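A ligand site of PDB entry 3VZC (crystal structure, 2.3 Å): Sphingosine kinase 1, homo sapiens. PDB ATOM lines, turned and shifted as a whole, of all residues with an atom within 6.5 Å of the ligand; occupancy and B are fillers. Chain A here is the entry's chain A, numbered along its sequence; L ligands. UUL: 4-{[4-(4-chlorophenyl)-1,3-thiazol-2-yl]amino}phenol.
The backbone carbonyl oxygen (O) of Leu 256 sits at hydrogen-bond distance from the backbone NH (N) of Val 287, at 2.8 Å. The backbone carbonyl oxygen (O) of Leu 258 sits at hydrogen-bond distance from the backbone NH (N) of Phe 285, at 2.7 Å. The backbone carbonyl oxygen (O) of Phe 189 lies within hydrogen-bond range of the side-chain hydroxyl (OG1) of Thr 193, at 2.9 Å. A ring nitrogen (NE2) of His 308 lies within hydrogen-bond range of the backbone carbonyl oxygen (O) of Ala 271 (2.9 Å).
Residues that only touch the ligand: Phe 285 (3.2 Å), Phe 170 (3.3 Å), Leu 296 (3.4 Å), Phe 300 (3.4 Å), Val 174 (3.6 Å), Ile 171 (3.6 Å), Met 269 (3.7 Å), Met 303 (3.7 Å), His 308 (3.7 Å), Phe 189 (3.8 Å), Leu 265 (3.8 Å), Leu 258 (3.96 Å) and Leu 256 (3.97 Å). Hydrophobic or aromatic side chains within 4 Å of the ligand: Phe 170, Ile 171, Val 174, Phe 189, Leu 256, Leu 258, Leu 265, Met 269, Phe 285, Leu 296, Phe 300, Met 303 and His 308. 15 residues have an atom within 4 Å of the ligand: Phe 170, Ile 171, Val 174, Asp 175, Phe 189, Thr 193, Leu 256, Leu 258, Leu 265, Met 269, Phe 285, Leu 296, Phe 300, Met 303 and His 308. The nearest printed residue that does not touch the ligand is Ala 271 (4.1 Å).
The side-chain hydroxyl (OG1) of Thr 193 is in hydrogen-bond range of a nitrogen (N6) of the ligand (2.9 Å). O20 of the ligand is in hydrogen-bond range of OD2 of Asp 175 (2.5 Å).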
ATOM      1  N   PHE A 170      25.928   2.447 -27.487  1.00  0.00           N
ATOM      2  CA  PHE A 170      27.093   2.044 -26.681  1.00  0.00           C
ATOM      3  C   PHE A 170      27.820   0.812 -27.221  1.00  0.00           C
ATOM      4  O   PHE A 170      29.034   0.859 -27.465  1.00  0.00           O
ATOM      5  CB  PHE A 170      26.664   1.834 -25.230  1.00  0.00           C
ATOM      6  CG  PHE A 170      27.807   1.621 -24.270  1.00  0.00           C
ATOM      7  CD1 PHE A 170      28.219   0.333 -23.935  1.00  0.00           C
ATOM      8  CD2 PHE A 170      28.439   2.706 -23.670  1.00  0.00           C
ATOM      9  CE1 PHE A 170      29.248   0.129 -23.029  1.00  0.00           C
ATOM     10  CE2 PHE A 170      29.479   2.520 -22.767  1.00  0.00           C
ATOM     11  CZ  PHE A 170      29.882   1.224 -22.451  1.00  0.00           C
ATOM     12  N   ILE A 171      27.086  -0.282 -27.423  1.00  0.00           N
ATOM     13  CA  ILE A 171      27.668  -1.513 -27.979  1.00  0.00           C
ATOM     14  C   ILE A 171      28.299  -1.307 -29.372  1.00  0.00           C
ATOM     15  O   ILE A 171      29.352  -1.871 -29.664  1.00  0.00           O
ATOM     16  CB  ILE A 171      26.617  -2.630 -28.077  1.00  0.00           C
ATOM     17  CG1 ILE A 171      26.132  -3.022 -26.687  1.00  0.00           C
ATOM     18  CG2 ILE A 171      27.152  -3.842 -28.835  1.00  0.00           C
ATOM     19  CD1 ILE A 171      25.171  -4.191 -26.737  1.00  0.00           C
ATOM     20  N   ALA A 172      27.668  -0.500 -30.212  1.00  0.00           N
ATOM     21  CA  ALA A 172      28.233  -0.235 -31.523  1.00  0.00           C
ATOM     22  C   ALA A 172      29.522   0.556 -31.394  1.00  0.00           C
ATOM     23  O   ALA A 172      30.539   0.217 -32.017  1.00  0.00           O
ATOM     24  CB  ALA A 172      27.244   0.495 -32.419  1.00  0.00           C
ATOM     25  N   VAL A 174      31.662   0.695 -29.055  1.00  0.00           N
ATOM     26  CA  VAL A 174      32.721  -0.137 -28.475  1.00  0.00           C
ATOM     27  C   VAL A 174      33.238  -1.174 -29.478  1.00  0.00           C
ATOM     28  O   VAL A 174      34.447  -1.403 -29.568  1.00  0.00           O
ATOM     29  CB  VAL A 174      32.243  -0.786 -27.156  1.00  0.00           C
ATOM     30  CG1 VAL A 174      33.165  -1.905 -26.718  1.00  0.00           C
ATOM     31  CG2 VAL A 174      32.128   0.260 -26.053  1.00  0.00           C
ATOM     32  N   ASP A 175      32.336  -1.816 -30.229  1.00  0.00           N
ATOM     33  CA  ASP A 175      32.761  -2.715 -31.315  1.00  0.00           C
ATOM     34  C   ASP A 175      33.717  -2.007 -32.273  1.00  0.00           C
ATOM     35  O   ASP A 175      34.715  -2.588 -32.686  1.00  0.00           O
ATOM     36  CB  ASP A 175      31.554  -3.264 -32.084  1.00  0.00           C
ATOM     37  CG  ASP A 175      30.788  -4.348 -31.341  1.00  0.00           C
ATOM     38  OD1 ASP A 175      29.820  -4.867 -31.931  1.00  0.00           O
ATOM     39  OD2 ASP A 175      31.134  -4.688 -30.177  1.00  0.00           O
ATOM     40  N   PHE A 189      36.559  -6.101 -25.287  1.00  0.00           N
ATOM     41  CA  PHE A 189      35.216  -5.570 -25.096  1.00  0.00           C
ATOM     42  C   PHE A 189      35.039  -5.022 -23.696  1.00  0.00           C
ATOM     43  O   PHE A 189      34.426  -3.983 -23.517  1.00  0.00           O
ATOM     44  CB  PHE A 189      34.138  -6.610 -25.452  1.00  0.00           C
ATOM     45  CG  PHE A 189      34.111  -6.937 -26.915  1.00  0.00           C
ATOM     46  CD1 PHE A 189      33.871  -5.941 -27.863  1.00  0.00           C
ATOM     47  CD2 PHE A 189      34.349  -8.247 -27.351  1.00  0.00           C
ATOM     48  CE1 PHE A 189      33.848  -6.251 -29.224  1.00  0.00           C
ATOM     49  CE2 PHE A 189      34.335  -8.554 -28.706  1.00  0.00           C
ATOM     50  CZ  PHE A 189      34.096  -7.553 -29.642  1.00  0.00           C
ATOM     51  N   GLY A 192      37.163  -1.858 -23.715  1.00  0.00           N
ATOM     52  CA  GLY A 192      36.408  -0.862 -24.468  1.00  0.00           C
ATOM     53  C   GLY A 192      35.172  -0.346 -23.733  1.00  0.00           C
ATOM     54  O   GLY A 192      34.847   0.843 -23.782  1.00  0.00           O
ATOM     55  N   THR A 193      34.479  -1.263 -23.058  1.00  0.00           N
ATOM     56  CA  THR A 193      33.289  -0.889 -22.312  1.00  0.00           C
ATOM     57  C   THR A 193      33.699   0.042 -21.180  1.00  0.00           C
ATOM     58  O   THR A 193      33.072   1.079 -20.967  1.00  0.00           O
ATOM     59  CB  THR A 193      32.545  -2.129 -21.811  1.00  0.00           C
ATOM     60  OG1 THR A 193      31.878  -2.756 -22.914  1.00  0.00           O
ATOM     61  CG2 THR A 193      31.510  -1.781 -20.720  1.00  0.00           C
ATOM     62  N   LEU A 197      32.628   3.916 -20.937  1.00  0.00           N
ATOM     63  CA  LEU A 197      31.855   4.205 -19.736  1.00  0.00           C
ATOM     64  C   LEU A 197      32.294   5.523 -19.104  1.00  0.00           C
ATOM     65  O   LEU A 197      31.495   6.182 -18.459  1.00  0.00           O
ATOM     66  CB  LEU A 197      32.065   3.073 -18.732  1.00  0.00           C
ATOM     67  CG  LEU A 197      30.893   2.312 -18.119  1.00  0.00           C
ATOM     68  CD1 LEU A 197      29.720   2.203 -19.090  1.00  0.00           C
ATOM     69  CD2 LEU A 197      31.360   0.914 -17.728  1.00  0.00           C
ATOM     70  N   LEU A 256      21.875   2.264 -25.415  1.00  0.00           N
ATOM     71  CA  LEU A 256      21.978   1.229 -26.459  1.00  0.00           C
ATOM     72  C   LEU A 256      20.636   0.591 -26.866  1.00  0.00           C
ATOM     73  O   LEU A 256      19.684   0.511 -26.071  1.00  0.00           O
ATOM     74  CB  LEU A 256      22.967   0.120 -26.041  1.00  0.00           C
ATOM     75  CG  LEU A 256      22.494  -0.857 -24.948  1.00  0.00           C
ATOM     76  CD1 LEU A 256      21.681  -2.008 -25.534  1.00  0.00           C
ATOM     77  CD2 LEU A 256      23.660  -1.383 -24.113  1.00  0.00           C
ATOM     78  N   LEU A 258      19.621  -3.160 -28.972  1.00  0.00           N
ATOM     79  CA  LEU A 258      20.200  -4.406 -29.361  1.00  0.00           C
ATOM     80  C   LEU A 258      19.144  -5.380 -29.824  1.00  0.00           C
ATOM     81  O   LEU A 258      18.244  -5.777 -29.059  1.00  0.00           O
ATOM     82  CB  LEU A 258      21.023  -5.007 -28.201  1.00  0.00           C
ATOM     83  CG  LEU A 258      21.497  -6.466 -28.360  1.00  0.00           C
ATOM     84  CD1 LEU A 258      22.386  -6.624 -29.592  1.00  0.00           C
ATOM     85  CD2 LEU A 258      22.258  -6.894 -27.120  1.00  0.00           C
ATOM     86  N   LEU A 265      26.012 -12.690 -26.886  1.00  0.00           N
ATOM     87  CA  LEU A 265      26.643 -11.565 -27.586  1.00  0.00           C
ATOM     88  C   LEU A 265      28.146 -11.744 -27.806  1.00  0.00           C
ATOM     89  O   LEU A 265      28.778 -10.962 -28.502  1.00  0.00           O
ATOM     90  CB  LEU A 265      26.487 -10.309 -26.758  1.00  0.00           C
ATOM     91  CG  LEU A 265      25.550  -9.161 -27.058  1.00  0.00           C
ATOM     92  CD1 LEU A 265      25.832  -8.122 -25.973  1.00  0.00           C
ATOM     93  CD2 LEU A 265      25.765  -8.585 -28.453  1.00  0.00           C
ATOM     94  N   MET A 269      29.462 -13.600 -22.783  1.00  0.00           N
ATOM     95  CA  MET A 269      28.360 -12.673 -22.634  1.00  0.00           C
ATOM     96  C   MET A 269      27.048 -13.434 -22.888  1.00  0.00           C
ATOM     97  O   MET A 269      26.581 -13.532 -24.017  1.00  0.00           O
ATOM     98  CB  MET A 269      28.522 -11.469 -23.582  1.00  0.00           C
ATOM     99  CG  MET A 269      29.744 -10.594 -23.280  1.00  0.00           C
ATOM    100  SD  MET A 269      29.867  -9.085 -24.257  1.00  0.00           S
ATOM    101  CE  MET A 269      30.867  -9.645 -25.635  1.00  0.00           C
ATOM    102  N   ALA A 271      23.894 -12.925 -22.881  1.00  0.00           N
ATOM    103  CA  ALA A 271      23.026 -11.730 -22.910  1.00  0.00           C
ATOM    104  C   ALA A 271      21.548 -12.045 -22.851  1.00  0.00           C
ATOM    105  O   ALA A 271      20.759 -11.216 -22.403  1.00  0.00           O
ATOM    106  CB  ALA A 271      23.325 -10.879 -24.142  1.00  0.00           C
ATOM    107  N   ALA A 272      21.167 -13.243 -23.296  1.00  0.00           N
ATOM    108  CA  ALA A 272      19.765 -13.606 -23.381  1.00  0.00           C
ATOM    109  C   ALA A 272      19.481 -14.927 -22.686  1.00  0.00           C
ATOM    110  O   ALA A 272      19.304 -15.956 -23.358  1.00  0.00           O
ATOM    111  CB  ALA A 272      19.309 -13.652 -24.823  1.00  0.00           C
ATOM    112  N   PHE A 285      16.576  -5.668 -26.964  1.00  0.00           N
ATOM    113  CA  PHE A 285      16.975  -5.040 -25.711  1.00  0.00           C
ATOM    114  C   PHE A 285      17.206  -3.574 -25.980  1.00  0.00           C
ATOM    115  O   PHE A 285      17.787  -3.206 -27.002  1.00  0.00           O
ATOM    116  CB  PHE A 285      18.288  -5.622 -25.182  1.00  0.00           C
ATOM    117  CG  PHE A 285      18.206  -7.072 -24.796  1.00  0.00           C
ATOM    118  CD1 PHE A 285      17.947  -7.427 -23.483  1.00  0.00           C
ATOM    119  CD2 PHE A 285      18.433  -8.075 -25.727  1.00  0.00           C
ATOM    120  CE1 PHE A 285      17.907  -8.760 -23.097  1.00  0.00           C
ATOM    121  CE2 PHE A 285      18.391  -9.413 -25.354  1.00  0.00           C
ATOM    122  CZ  PHE A 285      18.128  -9.756 -24.039  1.00  0.00           C
ATOM    123  N   VAL A 287      18.422   0.102 -23.605  1.00  0.00           N
ATOM    124  CA  VAL A 287      18.709   0.777 -22.354  1.00  0.00           C
ATOM    125  C   VAL A 287      18.399   2.255 -22.526  1.00  0.00           C
ATOM    126  O   VAL A 287      19.017   2.945 -23.357  1.00  0.00           O
ATOM    127  CB  VAL A 287      20.167   0.551 -21.854  1.00  0.00           C
ATOM    128  CG1 VAL A 287      20.415   1.313 -20.563  1.00  0.00           C
ATOM    129  CG2 VAL A 287      20.420  -0.925 -21.613  1.00  0.00           C
ATOM    130  N   LEU A 296      25.433   0.273 -15.447  1.00  0.00           N
ATOM    131  CA  LEU A 296      25.758  -0.231 -16.767  1.00  0.00           C
ATOM    132  C   LEU A 296      26.826  -1.310 -16.628  1.00  0.00           C
ATOM    133  O   LEU A 296      26.657  -2.432 -17.144  1.00  0.00           O
ATOM    134  CB  LEU A 296      26.232   0.910 -17.680  1.00  0.00           C
ATOM    135  CG  LEU A 296      25.487   1.087 -19.018  1.00  0.00           C
ATOM    136  CD1 LEU A 296      26.241   1.993 -19.973  1.00  0.00           C
ATOM    137  CD2 LEU A 296      25.115  -0.226 -19.700  1.00  0.00           C
ATOM    138  N   LEU A 297      27.884  -1.000 -15.872  1.00  0.00           N
ATOM    139  CA  LEU A 297      29.018  -1.916 -15.680  1.00  0.00           C
ATOM    140  C   LEU A 297      28.591  -3.167 -14.956  1.00  0.00           C
ATOM    141  O   LEU A 297      28.966  -4.292 -15.334  1.00  0.00           O
ATOM    142  CB  LEU A 297      30.160  -1.236 -14.929  1.00  0.00           C
ATOM    143  CG  LEU A 297      31.468  -2.027 -14.819  1.00  0.00           C
ATOM    144  CD1 LEU A 297      32.016  -2.440 -16.179  1.00  0.00           C
ATOM    145  CD2 LEU A 297      32.499  -1.228 -14.043  1.00  0.00           C
ATOM    146  N   LEU A 299      25.587  -4.357 -15.022  1.00  0.00           N
ATOM    147  CA  LEU A 299      24.767  -5.120 -15.968  1.00  0.00           C
ATOM    148  C   LEU A 299      25.684  -5.894 -16.934  1.00  0.00           C
ATOM    149  O   LEU A 299      25.450  -7.079 -17.228  1.00  0.00           O
ATOM    150  CB  LEU A 299      23.757  -4.225 -16.736  1.00  0.00           C
ATOM    151  CG  LEU A 299      22.559  -3.535 -16.028  1.00  0.00           C
ATOM    152  CD1 LEU A 299      21.767  -2.640 -16.966  1.00  0.00           C
ATOM    153  CD2 LEU A 299      21.612  -4.521 -15.329  1.00  0.00           C
ATOM    154  N   PHE A 300      26.728  -5.218 -17.370  1.00  0.00           N
ATOM    155  CA  PHE A 300      27.776  -5.800 -18.178  1.00  0.00           C
ATOM    156  C   PHE A 300      28.442  -7.024 -17.547  1.00  0.00           C
ATOM    157  O   PHE A 300      28.577  -8.055 -18.199  1.00  0.00           O
ATOM    158  CB  PHE A 300      28.843  -4.768 -18.541  1.00  0.00           C
ATOM    159  CG  PHE A 300      29.915  -5.306 -19.453  1.00  0.00           C
ATOM    160  CD1 PHE A 300      29.646  -5.522 -20.808  1.00  0.00           C
ATOM    161  CD2 PHE A 300      31.179  -5.591 -18.971  1.00  0.00           C
ATOM    162  CE1 PHE A 300      30.621  -6.011 -21.646  1.00  0.00           C
ATOM    163  CE2 PHE A 300      32.167  -6.083 -19.809  1.00  0.00           C
ATOM    164  CZ  PHE A 300      31.885  -6.290 -21.152  1.00  0.00           C
ATOM    165  N   MET A 303      26.327 -10.086 -17.023  1.00  0.00           N
ATOM    166  CA  MET A 303      26.095 -10.717 -18.318  1.00  0.00           C
ATOM    167  C   MET A 303      26.917 -11.980 -18.504  1.00  0.00           C
ATOM    168  O   MET A 303      26.451 -12.940 -19.146  1.00  0.00           O
ATOM    169  CB  MET A 303      26.360  -9.725 -19.450  1.00  0.00           C
ATOM    170  CG  MET A 303      25.967 -10.199 -20.845  1.00  0.00           C
ATOM    171  SD  MET A 303      25.623  -8.827 -21.954  1.00  0.00           S
ATOM    172  CE  MET A 303      27.162  -7.922 -22.029  1.00  0.00           C
ATOM    173  N   HIS A 308      22.115 -10.515 -15.398  1.00  0.00           N
ATOM    174  CA  HIS A 308      21.778  -9.093 -15.491  1.00  0.00           C
ATOM    175  C   HIS A 308      20.297  -8.783 -15.427  1.00  0.00           C
ATOM    176  O   HIS A 308      19.918  -7.711 -14.934  1.00  0.00           O
ATOM    177  CB  HIS A 308      22.407  -8.481 -16.729  1.00  0.00           C
ATOM    178  CG  HIS A 308      22.081  -9.204 -17.999  1.00  0.00           C
ATOM    179  ND1 HIS A 308      22.413 -10.484 -18.207  1.00  0.00           N
ATOM    180  CD2 HIS A 308      21.397  -8.786 -19.139  1.00  0.00           C
ATOM    181  CE1 HIS A 308      21.983 -10.866 -19.421  1.00  0.00           C
ATOM    182  NE2 HIS A 308      21.363  -9.823 -19.983  1.00  0.00           N
ATOM    183  N   MET A 309      19.444  -9.692 -15.898  1.00  0.00           N
ATOM    184  CA  MET A 309      17.977  -9.511 -15.834  1.00  0.00           C
ATOM    185  C   MET A 309      17.452  -9.601 -14.393  1.00  0.00           C
ATOM    186  O   MET A 309      16.344  -9.151 -14.100  1.00  0.00           O
ATOM    187  CB  MET A 309      17.238 -10.523 -16.736  1.00  0.00           C
ATOM    188  CG  MET A 309      17.627 -10.553 -18.222  1.00  0.00           C
ATOM    189  SD  MET A 309      17.656  -8.947 -19.078  1.00  0.00           S
ATOM    190  CE  MET A 309      15.952  -8.405 -18.976  1.00  0.00           C
ATOM    191  N   LEU A 316      16.582  -0.936 -18.315  1.00  0.00           N
ATOM    192  CA  LEU A 316      16.794  -2.006 -19.291  1.00  0.00           C
ATOM    193  C   LEU A 316      15.482  -2.640 -19.656  1.00  0.00           C
ATOM    194  O   LEU A 316      14.772  -3.125 -18.782  1.00  0.00           O
ATOM    195  CB  LEU A 316      17.753  -3.087 -18.765  1.00  0.00           C
ATOM    196  CG  LEU A 316      17.961  -4.334 -19.643  1.00  0.00           C
ATOM    197  CD1 LEU A 316      18.637  -3.994 -20.982  1.00  0.00           C
ATOM    198  CD2 LEU A 316      18.741  -5.410 -18.900  1.00  0.00           C
HETATM  199  C16 UUL L   1      28.813  -5.381 -25.029  1.00  0.00           C
HETATM  200  C19 UUL L   1      29.059  -6.076 -26.220  1.00  0.00           C
HETATM  201  C12 UUL L   1      29.862  -5.494 -27.200  1.00  0.00           C
HETATM  202  O20 UUL L   1      30.126  -6.112 -28.369  1.00  0.00           O
HETATM  203  C18 UUL L   1      30.398  -4.223 -27.009  1.00  0.00           C
HETATM  204  C17 UUL L   1      30.133  -3.549 -25.821  1.00  0.00           C
HETATM  205  C10 UUL L   1      29.350  -4.103 -24.825  1.00  0.00           C
HETATM  206  N6  UUL L   1      29.159  -3.358 -23.712  1.00  0.00           N
HETATM  207  C2  UUL L   1      28.072  -3.362 -22.917  1.00  0.00           C
HETATM  208  N1  UUL L   1      26.975  -4.105 -23.069  1.00  0.00           N
HETATM  209  S4  UUL L   1      27.854  -2.418 -21.504  1.00  0.00           S
HETATM  210  C5  UUL L   1      26.321  -3.042 -21.157  1.00  0.00           C
HETATM  211  C3  UUL L   1      26.008  -3.933 -22.129  1.00  0.00           C
HETATM  212  C7  UUL L   1      24.807  -4.656 -22.176  1.00  0.00           C
HETATM  213  C8  UUL L   1      24.564  -5.463 -23.286  1.00  0.00           C
HETATM  214  C14 UUL L   1      23.398  -6.220 -23.384  1.00  0.00           C
HETATM  215  C11 UUL L   1      22.460  -6.147 -22.358  1.00  0.00           C
HETATM  216 CL   UUL L   1      21.007  -7.087 -22.489  1.00  0.00          CL
HETATM  217  C13 UUL L   1      22.696  -5.344 -21.237  1.00  0.00           C
HETATM  218  C9  UUL L   1      23.867  -4.592 -21.145  1.00  0.00           C
